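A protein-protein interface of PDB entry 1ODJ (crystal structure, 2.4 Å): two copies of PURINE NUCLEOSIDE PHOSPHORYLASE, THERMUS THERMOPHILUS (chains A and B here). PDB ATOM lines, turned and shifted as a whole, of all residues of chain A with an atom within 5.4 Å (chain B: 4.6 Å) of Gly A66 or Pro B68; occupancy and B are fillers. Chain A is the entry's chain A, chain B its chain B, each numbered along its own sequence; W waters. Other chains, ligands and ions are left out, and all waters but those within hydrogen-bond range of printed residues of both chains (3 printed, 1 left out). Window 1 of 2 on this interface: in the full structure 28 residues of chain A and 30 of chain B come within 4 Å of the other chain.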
ATOM      1  N   THR A  63       4.232  26.027  -2.399  1.00  0.00           N
ATOM      2  CA  THR A  63       3.166  25.254  -1.760  1.00  0.00           C
ATOM      3  C   THR A  63       3.206  25.361  -0.239  1.00  0.00           C
ATOM      4  O   THR A  63       2.171  25.394   0.409  1.00  0.00           O
ATOM      5  CB  THR A  63       3.283  23.757  -2.117  1.00  0.00           C
ATOM      6  OG1 THR A  63       4.543  23.267  -1.653  1.00  0.00           O
ATOM      7  CG2 THR A  63       3.193  23.538  -3.632  1.00  0.00           C
ATOM      8  N   GLY A  64       4.412  25.421   0.321  1.00  0.00           N
ATOM      9  CA  GLY A  64       4.565  25.503   1.762  1.00  0.00           C
ATOM     10  C   GLY A  64       4.931  24.107   2.216  1.00  0.00           C
ATOM     11  O   GLY A  64       5.011  23.211   1.381  1.00  0.00           O
ATOM     12  N   MET A  65       5.166  23.909   3.509  1.00  0.00           N
ATOM     13  CA  MET A  65       5.508  22.582   4.011  1.00  0.00           C
ATOM     14  C   MET A  65       4.274  21.859   4.539  1.00  0.00           C
ATOM     15  O   MET A  65       3.528  22.399   5.357  1.00  0.00           O
ATOM     16  CB  MET A  65       6.570  22.675   5.114  1.00  0.00           C
ATOM     17  CG  MET A  65       7.919  23.213   4.645  1.00  0.00           C
ATOM     18  SD  MET A  65       9.232  23.035   5.879  1.00  0.00           S
ATOM     19  CE  MET A  65       8.829  24.399   6.945  1.00  0.00           C
ATOM     20  N   GLY A  66       4.056  20.636   4.060  1.00  0.00           N
ATOM     21  CA  GLY A  66       2.905  19.869   4.507  1.00  0.00           C
ATOM     22  C   GLY A  66       1.768  19.763   3.507  1.00  0.00           C
ATOM     23  O   GLY A  66       1.495  20.686   2.733  1.00  0.00           O
ATOM     24  N   THR A  67       1.093  18.619   3.523  1.00  0.00           N
ATOM     25  CA  THR A  67      -0.029  18.392   2.628  1.00  0.00           C
ATOM     26  C   THR A  67      -1.175  19.371   2.850  1.00  0.00           C
ATOM     27  O   THR A  67      -1.849  19.734   1.897  1.00  0.00           O
ATOM     28  CB  THR A  67      -0.570  16.957   2.747  1.00  0.00           C
ATOM     29  OG1 THR A  67      -0.807  16.646   4.121  1.00  0.00           O
ATOM     30  CG2 THR A  67       0.425  15.968   2.155  1.00  0.00           C
ATOM     31  N   PRO A  68      -1.414  19.819   4.102  1.00  0.00           N
ATOM     32  CA  PRO A  68      -2.523  20.770   4.309  1.00  0.00           C
ATOM     33  C   PRO A  68      -2.298  22.039   3.495  1.00  0.00           C
ATOM     34  O   PRO A  68      -3.186  22.512   2.790  1.00  0.00           O
ATOM     35  CB  PRO A  68      -2.473  21.058   5.814  1.00  0.00           C
ATOM     36  CG  PRO A  68      -1.823  19.828   6.392  1.00  0.00           C
ATOM     37  CD  PRO A  68      -0.742  19.511   5.378  1.00  0.00           C
ATOM     38  N   SER A  69      -1.097  22.584   3.620  1.00  0.00           N
ATOM     39  CA  SER A  69      -0.706  23.793   2.921  1.00  0.00           C
ATOM     40  C   SER A  69      -0.691  23.523   1.416  1.00  0.00           C
ATOM     41  O   SER A  69      -1.290  24.263   0.627  1.00  0.00           O
ATOM     42  CB  SER A  69       0.687  24.225   3.414  1.00  0.00           C
ATOM     43  OG  SER A  69       1.158  25.406   2.788  1.00  0.00           O
ATOM     44  N   ALA A  70       0.004  22.455   1.035  1.00  0.00           N
ATOM     45  CA  ALA A  70       0.126  22.042  -0.359  1.00  0.00           C
ATOM     46  C   ALA A  70      -1.246  21.832  -0.964  1.00  0.00           C
ATOM     47  O   ALA A  70      -1.473  22.218  -2.109  1.00  0.00           O
ATOM     48  CB  ALA A  70       0.957  20.742  -0.466  1.00  0.00           C
ATOM     49  N   ALA A  71      -2.161  21.230  -0.199  1.00  0.00           N
ATOM     50  CA  ALA A  71      -3.523  20.976  -0.682  1.00  0.00           C
ATOM     51  C   ALA A  71      -4.235  22.286  -0.980  1.00  0.00           C
ATOM     52  O   ALA A  71      -4.869  22.433  -2.024  1.00  0.00           O
ATOM     53  CB  ALA A  71      -4.326  20.170   0.344  1.00  0.00           C
ATOM     54  N   GLU A 156       4.670  12.193   4.972  1.00  0.00           N
ATOM     55  CA  GLU A 156       4.264  12.247   6.367  1.00  0.00           C
ATOM     56  C   GLU A 156       3.867  13.661   6.800  1.00  0.00           C
ATOM     57  O   GLU A 156       4.005  14.618   6.038  1.00  0.00           O
ATOM     58  CB  GLU A 156       5.365  11.692   7.284  1.00  0.00           C
ATOM     59  CG  GLU A 156       6.718  12.375   7.171  1.00  0.00           C
ATOM     60  CD  GLU A 156       7.745  11.778   8.130  1.00  0.00           C
ATOM     61  OE1 GLU A 156       8.907  12.233   8.116  1.00  0.00           O
ATOM     62  OE2 GLU A 156       7.398  10.856   8.903  1.00  0.00           O
ATOM     63  N   ASP A 157       3.367  13.770   8.028  1.00  0.00           N
ATOM     64  CA  ASP A 157       2.925  15.036   8.606  1.00  0.00           C
ATOM     65  C   ASP A 157       3.904  15.591   9.630  1.00  0.00           C
ATOM     66  O   ASP A 157       4.181  16.783   9.652  1.00  0.00           O
ATOM     67  CB  ASP A 157       1.567  14.847   9.283  1.00  0.00           C
ATOM     68  CG  ASP A 157       0.419  14.916   8.307  1.00  0.00           C
ATOM     69  OD1 ASP A 157      -0.686  14.443   8.652  1.00  0.00           O
ATOM     70  OD2 ASP A 157       0.612  15.456   7.196  1.00  0.00           O
ATOM     71  N   ALA A 158       4.411  14.710  10.482  1.00  0.00           N
ATOM     72  CA  ALA A 158       5.326  15.088  11.542  1.00  0.00           C
ATOM     73  C   ALA A 158       6.768  14.817  11.177  1.00  0.00           C
ATOM     74  O   ALA A 158       7.249  13.695  11.323  1.00  0.00           O
ATOM     75  CB  ALA A 158       4.970  14.338  12.813  1.00  0.00           C
ATOM     76  N   MET A 180       6.867  15.760   2.319  1.00  0.00           N
ATOM     77  CA  MET A 180       5.602  16.207   2.904  1.00  0.00           C
ATOM     78  C   MET A 180       4.572  16.870   1.994  1.00  0.00           C
ATOM     79  O   MET A 180       3.898  17.801   2.423  1.00  0.00           O
ATOM     80  CB  MET A 180       5.897  17.150   4.089  1.00  0.00           C
ATOM     81  CG  MET A 180       6.464  16.440   5.328  1.00  0.00           C
ATOM     82  SD  MET A 180       7.240  17.518   6.600  1.00  0.00           S
ATOM     83  CE  MET A 180       5.812  18.577   7.082  1.00  0.00           C
ATOM     84  N   GLU A 181       4.437  16.412   0.749  1.00  0.00           N
ATOM     85  CA  GLU A 181       3.447  16.999  -0.162  1.00  0.00           C
ATOM     86  C   GLU A 181       2.875  16.081  -1.218  1.00  0.00           C
ATOM     87  O   GLU A 181       1.680  16.148  -1.503  1.00  0.00           O
ATOM     88  CB  GLU A 181       4.010  18.223  -0.871  1.00  0.00           C
ATOM     89  CG  GLU A 181       4.134  19.428   0.013  1.00  0.00           C
ATOM     90  CD  GLU A 181       5.409  19.400   0.789  1.00  0.00           C
ATOM     91  OE1 GLU A 181       5.508  20.134   1.800  1.00  0.00           O
ATOM     92  OE2 GLU A 181       6.313  18.641   0.371  1.00  0.00           O
ATOM     93  N   GLY B  66      -1.149  24.798   8.615  1.00  0.00           N
ATOM     94  CA  GLY B  66      -1.185  23.365   8.891  1.00  0.00           C
ATOM     95  C   GLY B  66      -0.250  22.891  10.000  1.00  0.00           C
ATOM     96  O   GLY B  66       0.838  23.449  10.176  1.00  0.00           O
ATOM     97  N   THR B  67      -0.652  21.846  10.728  1.00  0.00           N
ATOM     98  CA  THR B  67       0.188  21.337  11.807  1.00  0.00           C
ATOM     99  C   THR B  67       1.559  20.773  11.361  1.00  0.00           C
ATOM    100  O   THR B  67       2.544  20.828  12.116  1.00  0.00           O
ATOM    101  CB  THR B  67      -0.579  20.311  12.696  1.00  0.00           C
ATOM    102  OG1 THR B  67      -1.188  19.304  11.886  1.00  0.00           O
ATOM    103  CG2 THR B  67      -1.677  21.030  13.501  1.00  0.00           C
ATOM    104  N   PRO B  68       1.654  20.242  10.136  1.00  0.00           N
ATOM    105  CA  PRO B  68       2.970  19.730   9.745  1.00  0.00           C
ATOM    106  C   PRO B  68       4.001  20.862   9.777  1.00  0.00           C
ATOM    107  O   PRO B  68       5.086  20.726  10.327  1.00  0.00           O
ATOM    108  CB  PRO B  68       2.730  19.213   8.332  1.00  0.00           C
ATOM    109  CG  PRO B  68       1.320  18.739   8.386  1.00  0.00           C
ATOM    110  CD  PRO B  68       0.630  19.865   9.145  1.00  0.00           C
ATOM    111  N   SER B  69       3.646  21.987   9.181  1.00  0.00           N
ATOM    112  CA  SER B  69       4.542  23.133   9.149  1.00  0.00           C
ATOM    113  C   SER B  69       4.774  23.666  10.571  1.00  0.00           C
ATOM    114  O   SER B  69       5.917  23.881  10.997  1.00  0.00           O
ATOM    115  CB  SER B  69       3.943  24.240   8.266  1.00  0.00           C
ATOM    116  OG  SER B  69       4.823  25.338   8.175  1.00  0.00           O
ATOM    117  N   ALA B  70       3.670  23.851  11.292  1.00  0.00           N
ATOM    118  CA  ALA B  70       3.678  24.372  12.652  1.00  0.00           C
ATOM    119  C   ALA B  70       4.467  23.538  13.647  1.00  0.00           C
ATOM    120  O   ALA B  70       5.118  24.100  14.521  1.00  0.00           O
ATOM    121  CB  ALA B  70       2.243  24.552  13.144  1.00  0.00           C
ATOM    122  N   ALA B  71       4.416  22.211  13.538  1.00  0.00           N
ATOM    123  CA  ALA B  71       5.151  21.356  14.477  1.00  0.00           C
ATOM    124  C   ALA B  71       6.656  21.510  14.268  1.00  0.00           C
ATOM    125  O   ALA B  71       7.443  21.467  15.216  1.00  0.00           O
ATOM    126  CB  ALA B  71       4.745  19.904  14.304  1.00  0.00           C
ATOM    127  N   ILE B  72       7.057  21.702  13.021  1.00  0.00           N
ATOM    128  CA  ILE B  72       8.459  21.892  12.728  1.00  0.00           C
ATOM    129  C   ILE B  72       8.927  23.191  13.381  1.00  0.00           C
ATOM    130  O   ILE B  72       9.971  23.232  14.039  1.00  0.00           O
ATOM    131  CB  ILE B  72       8.701  21.990  11.227  1.00  0.00           C
ATOM    132  CG1 ILE B  72       8.595  20.593  10.600  1.00  0.00           C
ATOM    133  CG2 ILE B  72      10.044  22.655  10.967  1.00  0.00           C
ATOM    134  CD1 ILE B  72       8.525  20.620   9.100  1.00  0.00           C
ATOM    135  N   THR B 115      -0.830  15.232  11.955  1.00  0.00           N
ATOM    136  CA  THR B 115       0.398  15.521  12.682  1.00  0.00           C
ATOM    137  C   THR B 115       0.294  15.022  14.133  1.00  0.00           C
ATOM    138  O   THR B 115       1.182  14.301  14.618  1.00  0.00           O
ATOM    139  CB  THR B 115       0.710  17.034  12.684  1.00  0.00           C
ATOM    140  OG1 THR B 115       0.991  17.465  11.346  1.00  0.00           O
ATOM    141  CG2 THR B 115       1.920  17.329  13.569  1.00  0.00           C
HETATM  142  O   HOH W   1      -1.413  17.008   9.854  1.00  0.00           O
HETATM  143  O   HOH W   2       4.808  26.118   5.537  1.00  0.00           O
HETATM  144  O   HOH W   3       6.131  18.257  10.733  1.00  0.00           O
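Of the printed residues of chain B, Gly A66 touches Pro B68 (3.9 Å).
Of the printed residues of chain B, Pro A68 touches Pro B68 (3.7 Å).
Of the printed residues of chain B, Asp A157 touches Pro B68 (3.1 Å) and Thr B115 (3.4 Å).
Printed residues of chain B within 4 Å of Met A180: Pro B68 (3.4 Å) and Ile B72 (3.95 Å).
The nearest printed residue of chain B that does not touch Gly A66 is Ser B69 (5.2 Å).
The nearest residue of chain A that does not touch Pro B68 is Met A65 (4.4 Å).
Water W3 bridges O of Asp A157 and O of Pro B68.
Water W2 lies within hydrogen-bond range of OG of Ser B69 (2.8 Å) and N of Met A65 (3.0 Å).
Water W1 lies within hydrogen-bond range of N of Thr B115, OD1 of Asp A157 and OG1 of Thr B67.
The backbone NH (N) of Gly A66 sits at hydrogen-bond distance from the side-chain carboxylate (OE1) of Glu A181, at 2.7 Å.
OG1 of Thr B67 lies within hydrogen-bond range of OG1 of Thr B115.
N of Thr A67 lies within hydrogen-bond range of O of Met A180, at 3.1 Å.
The backbone NH (N) of Gly A66 sits close to the backbone carbonyl oxygen (O) of Met A180, at 3.3 Å.
The side-chain carboxylate (OD1) of Asp A157 sits at hydrogen-bond distance from the backbone NH (N) of Thr B115 (3.4 Å).
Gly A66 touches Pro B68, but with the chains exchanged Pro A68 does not touch Gly B66 (4.1 Å).
Pro B68 touches its own counterpart, Pro A68.
6 positions are printed for both chains.
Of the 14 printed residues of chain A, 5 touch a printed residue of chain B.
Hydrophobic or aromatic side chains of chain A that line the printed part of chain B: Pro A68 and Met A180.
Among the printed residues, no Asp or Glu carboxylate lies within 4 Å of a Lys or Arg side-chain nitrogen of the other chain.
Ser B69 touches Met A65.
CB of Pro B68 touches CA of Gly A66 (3.9 Å).
Pro B68 touches Pro A68 (CD to CG, 3.7 Å).
O of Asp A157 touches CB of Pro B68, 3.1 Å away.
Met A180 touches Pro B68.
Ile B72 touches Met A180 (CD1 to CE, 3.95 Å).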
